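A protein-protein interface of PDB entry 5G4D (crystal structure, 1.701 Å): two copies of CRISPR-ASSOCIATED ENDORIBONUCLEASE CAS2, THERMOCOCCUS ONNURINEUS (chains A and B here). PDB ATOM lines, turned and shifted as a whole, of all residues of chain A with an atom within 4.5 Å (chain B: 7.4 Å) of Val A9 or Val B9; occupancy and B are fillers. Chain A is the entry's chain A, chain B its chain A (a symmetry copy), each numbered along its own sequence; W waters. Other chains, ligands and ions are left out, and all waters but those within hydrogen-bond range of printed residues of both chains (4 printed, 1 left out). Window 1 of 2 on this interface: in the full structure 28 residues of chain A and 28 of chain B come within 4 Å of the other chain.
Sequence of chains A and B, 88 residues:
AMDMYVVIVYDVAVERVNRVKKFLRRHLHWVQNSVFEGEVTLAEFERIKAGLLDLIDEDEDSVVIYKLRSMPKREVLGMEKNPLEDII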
ATOM      1  N   VAL A   7      15.624 -34.901 -30.262  1.00  0.00           N
ATOM      2  CA  VAL A   7      15.145 -33.743 -29.509  1.00  0.00           C
ATOM      3  C   VAL A   7      14.392 -34.313 -28.327  1.00  0.00           C
ATOM      4  O   VAL A   7      13.460 -35.106 -28.514  1.00  0.00           O
ATOM      5  CB  VAL A   7      14.226 -32.820 -30.331  1.00  0.00           C
ATOM      6  CG1 VAL A   7      13.680 -31.694 -29.434  1.00  0.00           C
ATOM      7  CG2 VAL A   7      14.938 -32.264 -31.559  1.00  0.00           C
ATOM      8  N   ILE A   8      14.790 -33.930 -27.114  1.00  0.00           N
ATOM      9  CA  ILE A   8      14.181 -34.466 -25.902  1.00  0.00           C
ATOM     10  C   ILE A   8      13.494 -33.335 -25.152  1.00  0.00           C
ATOM     11  O   ILE A   8      14.115 -32.305 -24.861  1.00  0.00           O
ATOM     12  CB  ILE A   8      15.214 -35.156 -24.995  1.00  0.00           C
ATOM     13  CG1 ILE A   8      15.868 -36.316 -25.744  1.00  0.00           C
ATOM     14  CG2 ILE A   8      14.532 -35.645 -23.712  1.00  0.00           C
ATOM     15  CD1 ILE A   8      16.716 -37.201 -24.837  1.00  0.00           C
ATOM     16  N   VAL A   9      12.219 -33.530 -24.838  1.00  0.00           N
ATOM     17  CA  VAL A   9      11.461 -32.594 -24.008  1.00  0.00           C
ATOM     18  C   VAL A   9      10.958 -33.366 -22.799  1.00  0.00           C
ATOM     19  O   VAL A   9      10.635 -34.552 -22.905  1.00  0.00           O
ATOM     20  CB  VAL A   9      10.286 -31.954 -24.782  1.00  0.00           C
ATOM     21  CG1 VAL A   9      10.805 -31.157 -25.956  1.00  0.00           C
ATOM     22  CG2 VAL A   9       9.312 -33.030 -25.256  1.00  0.00           C
ATOM     23  N   TYR A  10      10.907 -32.714 -21.641  1.00  0.00           N
ATOM     24  CA  TYR A  10      10.501 -33.455 -20.450  1.00  0.00           C
ATOM     25  C   TYR A  10       9.667 -32.584 -19.525  1.00  0.00           C
ATOM     26  O   TYR A  10       9.835 -31.366 -19.446  1.00  0.00           O
ATOM     27  CB  TYR A  10      11.694 -34.044 -19.681  1.00  0.00           C
ATOM     28  CG  TYR A  10      12.760 -33.056 -19.268  1.00  0.00           C
ATOM     29  CD1 TYR A  10      13.832 -32.779 -20.100  1.00  0.00           C
ATOM     30  CD2 TYR A  10      12.708 -32.424 -18.027  1.00  0.00           C
ATOM     31  CE1 TYR A  10      14.811 -31.888 -19.737  1.00  0.00           C
ATOM     32  CE2 TYR A  10      13.695 -31.531 -17.643  1.00  0.00           C
ATOM     33  CZ  TYR A  10      14.747 -31.274 -18.499  1.00  0.00           C
ATOM     34  OH  TYR A  10      15.744 -30.395 -18.139  1.00  0.00           O
ATOM     35  N   GLN A  32      16.640 -24.861 -24.325  1.00  0.00           N
ATOM     36  CA  GLN A  32      15.954 -23.931 -23.434  1.00  0.00           C
ATOM     37  C   GLN A  32      15.420 -24.776 -22.289  1.00  0.00           C
ATOM     38  O   GLN A  32      15.767 -25.957 -22.166  1.00  0.00           O
ATOM     39  CB  GLN A  32      14.848 -23.157 -24.152  1.00  0.00           C
ATOM     40  CG  GLN A  32      13.912 -24.038 -24.954  1.00  0.00           C
ATOM     41  CD  GLN A  32      12.700 -23.285 -25.484  1.00  0.00           C
ATOM     42  OE1 GLN A  32      11.559 -23.652 -25.194  1.00  0.00           O
ATOM     43  NE2 GLN A  32      12.940 -22.230 -26.263  1.00  0.00           N
ATOM     44  N   SER A  34      13.926 -27.328 -20.262  1.00  0.00           N
ATOM     45  CA  SER A  34      13.366 -28.670 -20.434  1.00  0.00           C
ATOM     46  C   SER A  34      13.421 -29.154 -21.883  1.00  0.00           C
ATOM     47  O   SER A  34      12.647 -30.029 -22.279  1.00  0.00           O
ATOM     48  CB  SER A  34      11.935 -28.749 -19.901  1.00  0.00           C
ATOM     49  OG  SER A  34      11.872 -28.191 -18.603  1.00  0.00           O
ATOM     50  N   VAL A  35      14.345 -28.628 -22.681  1.00  0.00           N
ATOM     51  CA  VAL A  35      14.537 -29.091 -24.055  1.00  0.00           C
ATOM     52  C   VAL A  35      16.020 -29.311 -24.310  1.00  0.00           C
ATOM     53  O   VAL A  35      16.831 -28.416 -24.055  1.00  0.00           O
ATOM     54  CB  VAL A  35      13.988 -28.087 -25.082  1.00  0.00           C
ATOM     55  CG1 VAL A  35      14.152 -28.652 -26.510  1.00  0.00           C
ATOM     56  CG2 VAL A  35      12.531 -27.730 -24.764  1.00  0.00           C
ATOM     57  N   SER A  62       6.951 -37.299 -17.586  1.00  0.00           N
ATOM     58  CA  SER A  62       6.883 -37.668 -18.993  1.00  0.00           C
ATOM     59  C   SER A  62       8.081 -37.106 -19.741  1.00  0.00           C
ATOM     60  O   SER A  62       8.386 -35.914 -19.643  1.00  0.00           O
ATOM     61  CB  SER A  62       5.578 -37.185 -19.634  1.00  0.00           C
ATOM     62  OG  SER A  62       5.580 -35.783 -19.837  1.00  0.00           O
ATOM     63  N   VAL A  63       8.757 -37.974 -20.484  1.00  0.00           N
ATOM     64  CA  VAL A  63       9.846 -37.591 -21.371  1.00  0.00           C
ATOM     65  C   VAL A  63       9.457 -38.030 -22.774  1.00  0.00           C
ATOM     66  O   VAL A  63       9.034 -39.173 -22.971  1.00  0.00           O
ATOM     67  CB  VAL A  63      11.185 -38.234 -20.959  1.00  0.00           C
ATOM     68  CG1 VAL A  63      12.300 -37.724 -21.847  1.00  0.00           C
ATOM     69  CG2 VAL A  63      11.496 -37.993 -19.479  1.00  0.00           C
ATOM     70  N   VAL A  64       9.557 -37.120 -23.737  1.00  0.00           N
ATOM     71  CA  VAL A  64       9.314 -37.436 -25.143  1.00  0.00           C
ATOM     72  C   VAL A  64      10.634 -37.290 -25.882  1.00  0.00           C
ATOM     73  O   VAL A  64      11.275 -36.234 -25.821  1.00  0.00           O
ATOM     74  CB  VAL A  64       8.231 -36.540 -25.763  1.00  0.00           C
ATOM     75  CG1 VAL A  64       8.091 -36.834 -27.262  1.00  0.00           C
ATOM     76  CG2 VAL A  64       6.903 -36.749 -25.058  1.00  0.00           C
ATOM     77  N   TYR A  66      12.005 -37.326 -29.510  1.00  0.00           N
ATOM     78  CA  TYR A  66      11.829 -37.332 -30.960  1.00  0.00           C
ATOM     79  C   TYR A  66      13.087 -37.888 -31.607  1.00  0.00           C
ATOM     80  O   TYR A  66      14.195 -37.464 -31.266  1.00  0.00           O
ATOM     81  CB  TYR A  66      11.562 -35.915 -31.468  1.00  0.00           C
ATOM     82  CG  TYR A  66      10.269 -35.325 -30.949  1.00  0.00           C
ATOM     83  CD1 TYR A  66       9.058 -35.638 -31.550  1.00  0.00           C
ATOM     84  CD2 TYR A  66      10.262 -34.453 -29.857  1.00  0.00           C
ATOM     85  CE1 TYR A  66       7.872 -35.104 -31.083  1.00  0.00           C
ATOM     86  CE2 TYR A  66       9.082 -33.920 -29.373  1.00  0.00           C
ATOM     87  CZ  TYR A  66       7.889 -34.252 -29.998  1.00  0.00           C
ATOM     88  OH  TYR A  66       6.710 -33.726 -29.528  1.00  0.00           O
ATOM     89  N   VAL B   7       7.178 -29.003 -34.549  1.00  0.00           N
ATOM     90  CA  VAL B   7       7.222 -29.181 -33.098  1.00  0.00           C
ATOM     91  C   VAL B   7       7.633 -27.837 -32.538  1.00  0.00           C
ATOM     92  O   VAL B   7       8.678 -27.299 -32.927  1.00  0.00           O
ATOM     93  CB  VAL B   7       8.215 -30.270 -32.649  1.00  0.00           C
ATOM     94  CG1 VAL B   7       8.281 -30.313 -31.112  1.00  0.00           C
ATOM     95  CG2 VAL B   7       7.860 -31.632 -33.235  1.00  0.00           C
ATOM     96  N   ILE B   8       6.819 -27.281 -31.641  1.00  0.00           N
ATOM     97  CA  ILE B   8       7.079 -25.959 -31.084  1.00  0.00           C
ATOM     98  C   ILE B   8       7.324 -26.092 -29.589  1.00  0.00           C
ATOM     99  O   ILE B   8       6.503 -26.671 -28.866  1.00  0.00           O
ATOM    100  CB  ILE B   8       5.920 -24.983 -31.349  1.00  0.00           C
ATOM    101  CG1 ILE B   8       5.710 -24.826 -32.854  1.00  0.00           C
ATOM    102  CG2 ILE B   8       6.219 -23.631 -30.692  1.00  0.00           C
ATOM    103  CD1 ILE B   8       4.752 -23.692 -33.201  1.00  0.00           C
ATOM    104  N   VAL B   9       8.447 -25.552 -29.128  1.00  0.00           N
ATOM    105  CA  VAL B   9       8.760 -25.484 -27.701  1.00  0.00           C
ATOM    106  C   VAL B   9       8.955 -24.019 -27.349  1.00  0.00           C
ATOM    107  O   VAL B   9       9.460 -23.242 -28.165  1.00  0.00           O
ATOM    108  CB  VAL B   9      10.017 -26.310 -27.344  1.00  0.00           C
ATOM    109  CG1 VAL B   9       9.792 -27.770 -27.661  1.00  0.00           C
ATOM    110  CG2 VAL B   9      11.233 -25.781 -28.101  1.00  0.00           C
ATOM    111  N   TYR B  10       8.541 -23.622 -26.149  1.00  0.00           N
ATOM    112  CA  TYR B  10       8.648 -22.205 -25.818  1.00  0.00           C
ATOM    113  C   TYR B  10       9.011 -22.013 -24.355  1.00  0.00           C
ATOM    114  O   TYR B  10       8.656 -22.809 -23.484  1.00  0.00           O
ATOM    115  CB  TYR B  10       7.368 -21.420 -26.146  1.00  0.00           C
ATOM    116  CG  TYR B  10       6.097 -21.946 -25.521  1.00  0.00           C
ATOM    117  CD1 TYR B  10       5.318 -22.884 -26.177  1.00  0.00           C
ATOM    118  CD2 TYR B  10       5.661 -21.476 -24.284  1.00  0.00           C
ATOM    119  CE1 TYR B  10       4.159 -23.368 -25.624  1.00  0.00           C
ATOM    120  CE2 TYR B  10       4.487 -21.946 -23.719  1.00  0.00           C
ATOM    121  CZ  TYR B  10       3.737 -22.887 -24.398  1.00  0.00           C
ATOM    122  OH  TYR B  10       2.563 -23.366 -23.861  1.00  0.00           O
ATOM    123  N   ASP B  11       9.753 -20.941 -24.127  1.00  0.00           N
ATOM    124  CA  ASP B  11      10.250 -20.527 -22.820  1.00  0.00           C
ATOM    125  C   ASP B  11       9.826 -19.067 -22.710  1.00  0.00           C
ATOM    126  O   ASP B  11      10.491 -18.196 -23.277  1.00  0.00           O
ATOM    127  CB  ASP B  11      11.765 -20.705 -22.775  1.00  0.00           C
ATOM    128  CG  ASP B  11      12.321 -20.669 -21.386  1.00  0.00           C
ATOM    129  OD1 ASP B  11      11.715 -19.999 -20.522  1.00  0.00           O
ATOM    130  OD2 ASP B  11      13.372 -21.319 -21.171  1.00  0.00           O
ATOM    131  N   VAL B  12       8.702 -18.799 -22.041  1.00  0.00           N
ATOM    132  CA  VAL B  12       8.068 -17.478 -22.057  1.00  0.00           C
ATOM    133  C   VAL B  12       7.858 -17.037 -20.616  1.00  0.00           C
ATOM    134  O   VAL B  12       7.542 -17.860 -19.754  1.00  0.00           O
ATOM    135  CB  VAL B  12       6.723 -17.500 -22.813  1.00  0.00           C
ATOM    136  CG1 VAL B  12       6.005 -16.147 -22.712  1.00  0.00           C
ATOM    137  CG2 VAL B  12       6.942 -17.867 -24.298  1.00  0.00           C
ATOM    138  N   LEU B  24      -1.701 -21.482 -28.948  1.00  0.00           N
ATOM    139  CA  LEU B  24      -1.223 -22.661 -29.661  1.00  0.00           C
ATOM    140  C   LEU B  24      -2.216 -23.815 -29.573  1.00  0.00           C
ATOM    141  O   LEU B  24      -2.278 -24.647 -30.488  1.00  0.00           O
ATOM    142  CB  LEU B  24       0.156 -23.072 -29.137  1.00  0.00           C
ATOM    143  CG  LEU B  24       1.301 -22.144 -29.579  1.00  0.00           C
ATOM    144  CD1 LEU B  24       2.605 -22.596 -28.937  1.00  0.00           C
ATOM    145  CD2 LEU B  24       1.466 -22.072 -31.097  1.00  0.00           C
ATOM    146  N   VAL B  31       1.396 -31.436 -26.388  1.00  0.00           N
ATOM    147  CA  VAL B  31       2.152 -32.658 -26.076  1.00  0.00           C
ATOM    148  C   VAL B  31       2.412 -32.777 -24.583  1.00  0.00           C
ATOM    149  O   VAL B  31       2.167 -33.821 -23.970  1.00  0.00           O
ATOM    150  CB  VAL B  31       3.479 -32.674 -26.869  1.00  0.00           C
ATOM    151  CG1 VAL B  31       4.348 -33.893 -26.489  1.00  0.00           C
ATOM    152  CG2 VAL B  31       3.224 -32.613 -28.363  1.00  0.00           C
ATOM    153  N   GLN B  32       2.911 -31.707 -23.986  1.00  0.00           N
ATOM    154  CA  GLN B  32       3.139 -31.602 -22.548  1.00  0.00           C
ATOM    155  C   GLN B  32       3.393 -30.127 -22.279  1.00  0.00           C
ATOM    156  O   GLN B  32       3.197 -29.285 -23.163  1.00  0.00           O
ATOM    157  CB  GLN B  32       4.294 -32.488 -22.083  1.00  0.00           C
ATOM    158  CG  GLN B  32       5.552 -32.333 -22.913  1.00  0.00           C
ATOM    159  CD  GLN B  32       6.750 -33.054 -22.313  1.00  0.00           C
ATOM    160  OE1 GLN B  32       7.779 -32.434 -22.034  1.00  0.00           O
ATOM    161  NE2 GLN B  32       6.623 -34.366 -22.111  1.00  0.00           N
ATOM    162  N   ASN B  33       3.820 -29.807 -21.063  1.00  0.00           N
ATOM    163  CA  ASN B  33       4.056 -28.411 -20.728  1.00  0.00           C
ATOM    164  C   ASN B  33       5.005 -27.770 -21.731  1.00  0.00           C
ATOM    165  O   ASN B  33       6.129 -28.250 -21.936  1.00  0.00           O
ATOM    166  CB  ASN B  33       4.616 -28.284 -19.314  1.00  0.00           C
ATOM    167  CG  ASN B  33       4.809 -26.848 -18.914  1.00  0.00           C
ATOM    168  OD1 ASN B  33       5.932 -26.337 -18.905  1.00  0.00           O
ATOM    169  ND2 ASN B  33       3.705 -26.165 -18.622  1.00  0.00           N
ATOM    170  N   SER B  34       4.510 -26.722 -22.387  1.00  0.00           N
ATOM    171  CA  SER B  34       5.279 -25.853 -23.280  1.00  0.00           C
ATOM    172  C   SER B  34       5.758 -26.574 -24.540  1.00  0.00           C
ATOM    173  O   SER B  34       6.733 -26.154 -25.167  1.00  0.00           O
ATOM    174  CB  SER B  34       6.462 -25.214 -22.551  1.00  0.00           C
ATOM    175  OG  SER B  34       6.028 -24.651 -21.329  1.00  0.00           O
ATOM    176  N   VAL B  35       5.072 -27.637 -24.949  1.00  0.00           N
ATOM    177  CA  VAL B  35       5.396 -28.338 -26.191  1.00  0.00           C
ATOM    178  C   VAL B  35       4.118 -28.581 -26.980  1.00  0.00           C
ATOM    179  O   VAL B  35       3.150 -29.121 -26.436  1.00  0.00           O
ATOM    180  CB  VAL B  35       6.095 -29.681 -25.929  1.00  0.00           C
ATOM    181  CG1 VAL B  35       6.477 -30.347 -27.269  1.00  0.00           C
ATOM    182  CG2 VAL B  35       7.308 -29.489 -25.011  1.00  0.00           C
ATOM    183  N   PHE B  36       4.141 -28.234 -28.267  1.00  0.00           N
ATOM    184  CA  PHE B  36       3.037 -28.477 -29.194  1.00  0.00           C
ATOM    185  C   PHE B  36       3.576 -29.100 -30.475  1.00  0.00           C
ATOM    186  O   PHE B  36       4.747 -28.924 -30.831  1.00  0.00           O
ATOM    187  CB  PHE B  36       2.263 -27.180 -29.540  1.00  0.00           C
ATOM    188  CG  PHE B  36       1.418 -26.646 -28.408  1.00  0.00           C
ATOM    189  CD1 PHE B  36       1.993 -25.935 -27.373  1.00  0.00           C
ATOM    190  CD2 PHE B  36       0.042 -26.851 -28.395  1.00  0.00           C
ATOM    191  CE1 PHE B  36       1.218 -25.445 -26.311  1.00  0.00           C
ATOM    192  CE2 PHE B  36      -0.754 -26.360 -27.347  1.00  0.00           C
ATOM    193  CZ  PHE B  36      -0.166 -25.652 -26.311  1.00  0.00           C
ATOM    194  N   LEU B  52       2.336 -15.733 -32.507  1.00  0.00           N
ATOM    195  CA  LEU B  52       3.299 -15.845 -31.416  1.00  0.00           C
ATOM    196  C   LEU B  52       4.080 -14.548 -31.232  1.00  0.00           C
ATOM    197  O   LEU B  52       4.306 -14.108 -30.097  1.00  0.00           O
ATOM    198  CB  LEU B  52       4.247 -17.023 -31.676  1.00  0.00           C
ATOM    199  CG  LEU B  52       3.589 -18.391 -31.508  1.00  0.00           C
ATOM    200  CD1 LEU B  52       4.522 -19.465 -32.031  1.00  0.00           C
ATOM    201  CD2 LEU B  52       3.223 -18.668 -30.029  1.00  0.00           C
ATOM    202  N   SER B  62      11.606 -17.026 -25.683  1.00  0.00           N
ATOM    203  CA  SER B  62      12.171 -17.778 -26.795  1.00  0.00           C
ATOM    204  C   SER B  62      11.207 -18.867 -27.234  1.00  0.00           C
ATOM    205  O   SER B  62      10.721 -19.651 -26.413  1.00  0.00           O
ATOM    206  CB  SER B  62      13.530 -18.382 -26.427  1.00  0.00           C
ATOM    207  OG  SER B  62      13.394 -19.482 -25.545  1.00  0.00           O
ATOM    208  N   VAL B  63      10.933 -18.908 -28.532  1.00  0.00           N
ATOM    209  CA  VAL B  63      10.141 -19.960 -29.152  1.00  0.00           C
ATOM    210  C   VAL B  63      11.015 -20.616 -30.210  1.00  0.00           C
ATOM    211  O   VAL B  63      11.636 -19.919 -31.019  1.00  0.00           O
ATOM    212  CB  VAL B  63       8.846 -19.417 -29.787  1.00  0.00           C
ATOM    213  CG1 VAL B  63       8.011 -20.560 -30.324  1.00  0.00           C
ATOM    214  CG2 VAL B  63       8.049 -18.560 -28.798  1.00  0.00           C
ATOM    215  N   VAL B  64      11.099 -21.941 -30.182  1.00  0.00           N
ATOM    216  CA  VAL B  64      11.819 -22.703 -31.200  1.00  0.00           C
ATOM    217  C   VAL B  64      10.798 -23.521 -31.972  1.00  0.00           C
ATOM    218  O   VAL B  64      10.028 -24.286 -31.379  1.00  0.00           O
ATOM    219  CB  VAL B  64      12.905 -23.605 -30.593  1.00  0.00           C
ATOM    220  CG1 VAL B  64      13.556 -24.463 -31.686  1.00  0.00           C
ATOM    221  CG2 VAL B  64      13.954 -22.767 -29.885  1.00  0.00           C
ATOM    222  N   ILE B  65      10.774 -23.342 -33.288  1.00  0.00           N
ATOM    223  CA  ILE B  65       9.864 -24.062 -34.171  1.00  0.00           C
ATOM    224  C   ILE B  65      10.705 -25.010 -35.019  1.00  0.00           C
ATOM    225  O   ILE B  65      11.349 -24.590 -35.995  1.00  0.00           O
ATOM    226  CB  ILE B  65       9.045 -23.104 -35.046  1.00  0.00           C
ATOM    227  CG1 ILE B  65       8.325 -22.086 -34.156  1.00  0.00           C
ATOM    228  CG2 ILE B  65       8.068 -23.889 -35.916  1.00  0.00           C
ATOM    229  CD1 ILE B  65       7.589 -21.008 -34.943  1.00  0.00           C
ATOM    230  N   TYR B  66      10.674 -26.300 -34.675  1.00  0.00           N
ATOM    231  CA  TYR B  66      11.302 -27.314 -35.519  1.00  0.00           C
ATOM    232  C   TYR B  66      10.408 -27.579 -36.719  1.00  0.00           C
ATOM    233  O   TYR B  66       9.201 -27.779 -36.556  1.00  0.00           O
ATOM    234  CB  TYR B  66      11.513 -28.605 -34.728  1.00  0.00           C
ATOM    235  CG  TYR B  66      12.476 -28.450 -33.571  1.00  0.00           C
ATOM    236  CD1 TYR B  66      13.846 -28.497 -33.781  1.00  0.00           C
ATOM    237  CD2 TYR B  66      12.010 -28.256 -32.268  1.00  0.00           C
ATOM    238  CE1 TYR B  66      14.733 -28.357 -32.732  1.00  0.00           C
ATOM    239  CE2 TYR B  66      12.887 -28.104 -31.210  1.00  0.00           C
ATOM    240  CZ  TYR B  66      14.252 -28.158 -31.454  1.00  0.00           C
ATOM    241  OH  TYR B  66      15.132 -28.011 -30.409  1.00  0.00           O
ATOM    242  N   GLU B  75       9.703 -41.764 -28.887  1.00  0.00           N
ATOM    243  CA  GLU B  75       9.541 -42.692 -27.776  1.00  0.00           C
ATOM    244  C   GLU B  75       9.180 -41.893 -26.535  1.00  0.00           C
ATOM    245  O   GLU B  75       9.770 -40.844 -26.279  1.00  0.00           O
ATOM    246  CB  GLU B  75      10.816 -43.495 -27.524  1.00  0.00           C
ATOM    247  CG  GLU B  75      10.765 -44.296 -26.234  1.00  0.00           C
ATOM    248  CD  GLU B  75      11.721 -45.470 -26.213  1.00  0.00           C
ATOM    249  OE1 GLU B  75      12.642 -45.527 -27.064  1.00  0.00           O
ATOM    250  OE2 GLU B  75      11.535 -46.350 -25.340  1.00  0.00           O
ATOM    251  N   LEU B  77       8.888 -41.882 -22.410  1.00  0.00           N
ATOM    252  CA  LEU B  77       9.244 -42.478 -21.133  1.00  0.00           C
ATOM    253  C   LEU B  77       8.281 -41.953 -20.079  1.00  0.00           C
ATOM    254  O   LEU B  77       8.072 -40.742 -19.984  1.00  0.00           O
ATOM    255  CB  LEU B  77      10.685 -42.146 -20.735  1.00  0.00           C
ATOM    256  CG  LEU B  77      11.768 -42.359 -21.792  1.00  0.00           C
ATOM    257  CD1 LEU B  77      13.161 -42.054 -21.245  1.00  0.00           C
ATOM    258  CD2 LEU B  77      11.705 -43.777 -22.336  1.00  0.00           C
HETATM  259  O   HOH W   1       4.010 -36.158 -22.556  1.00  0.00           O
HETATM  260  O   HOH W   2      10.780 -24.633 -23.049  1.00  0.00           O
HETATM  261  O   HOH W   3       8.540 -28.606 -18.859  1.00  0.00           O
HETATM  262  O   HOH W   4      15.785 -20.960 -26.993  1.00  0.00           O
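Val A9 touches just these residues of chain B: Val B9 (3.9 Å), Gln B32 (3.4 Å) and Val B35 (3.9 Å).
Val B9 touches just these residues of chain A: Val A9, Gln A32 and Val A35.
Printed residues of chain A within 4 Å of Glu B75: Val A63 (3.8 Å) and Val A64 (3.6 Å).
Of the printed residues of chain B, Tyr A10 touches Gln B32.
Of the printed residues of chain B, Val A35 touches Val B9 (3.9 Å).
Printed residues of chain A within 4 Å of Gln B32: Val A9, Tyr A10, Ser A62 and Val A64.
Printed residues of chain A within 4 Å of Tyr B10: Gln A32.
The backbone NH (N) of Tyr A10 lies within hydrogen-bond range of the backbone carbonyl oxygen (O) of Ser A34.
The backbone NH (N) of Asp B11 lies within hydrogen-bond range of the backbone carbonyl oxygen (O) of Ser B62 (2.8 Å).
The backbone carbonyl oxygen (O) of Val A7 sits at hydrogen-bond distance from the backbone NH (N) of Tyr A66 (2.8 Å).
O of Val A9 lies within hydrogen-bond range of N of Val A64, 2.9 Å away.
The backbone NH (N) of Tyr B10 sits at hydrogen-bond distance from the backbone carbonyl oxygen (O) of Ser B34 (3.3 Å).
The backbone carbonyl oxygen (O) of Val B9 sits at hydrogen-bond distance from the backbone NH (N) of Val B64 (2.9 Å).
Val A9 touches its own counterpart, Val B9.
Val A9 touches Gln B32, and with the chains exchanged Gln A32 touches Val B9.
Gln A32 touches Ser B62, and with the chains exchanged Ser A62 touches Gln B32.
Gln A32 touches Val B64, and with the chains exchanged Val A64 touches Gln B32.
Water W2 lies within hydrogen-bond range of the side-chain amide oxygen of Gln A32 and the backbone carbonyl oxygen of Tyr B10.
Water W3 lies within hydrogen-bond range of O of Tyr A10 (3.1 Å), OG of Ser A34 (3.4 Å) and OD1 of Asn B33 (3.5 Å).
Water W4 lies within hydrogen-bond range of the side-chain hydroxyl (OG) of Ser B62 (3.2 Å) and the side-chain amide nitrogen (NE2) of Gln A32 (3.2 Å).
Water W1 lies within hydrogen-bond range of the side-chain hydroxyl of Ser A62 (3.2 Å), the side-chain amide nitrogen of Gln B32 (3.2 Å) and the backbone carbonyl oxygen of Val B31 (3.3 Å).
Printed residues of chain B that touch a printed residue of chain A: Val B9, Tyr B10, Asp B11, Val B31, Gln B32, Val B35, Ser B62, Val B64, Glu B75 and Leu B77.
Of the 11 printed residues of chain A, 8 touch a printed residue of chain B.
Hydrophobic or aromatic side chains of chain A that line the printed part of chain B: Val A9, Val A35, Val A63, Val A64 and Tyr A66.
Among the printed residues, no Asp or Glu carboxylate lies within 4 Å of a Lys or Arg side-chain nitrogen of the other chain.
The side-chain amide nitrogen (NE2) of Gln A32 is in hydrogen-bond range of the side-chain hydroxyl (OG) of Ser B62 (2.9 Å).
The side-chain hydroxyl (OG) of Ser A62 sits at hydrogen-bond distance from the side-chain amide nitrogen (NE2) of Gln B32 (2.9 Å).
The backbone NH (N) of Tyr A10 lies close to the side-chain amide oxygen (OE1) of Gln B32 (3.2 Å).
The side-chain amide oxygen (OE1) of Gln A32 is in hydrogen-bond range of the backbone NH (N) of Asp B11 (3.4 Å).
The side-chain amide oxygen (OE1) of Gln A32 lies close to the backbone NH (N) of Tyr B10, at 3.2 Å.
The backbone NH of Leu B77 is in hydrogen-bond range of the backbone carbonyl oxygen of Val A63 (2.8 Å).
Among the printed residues, merely in contact across the chains: Val A9 with Val B9, Val A9 with Gln B32, Val A9 with Val B35, Gln A32 with Val B9, Gln A32 with Val B64, Val A35 with Val B9, Ser A62 with Leu B77, Val A63 with Glu B75, Val A64 with Gln B32, Val A64 with Glu B75 and Tyr A66 with Val B31.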
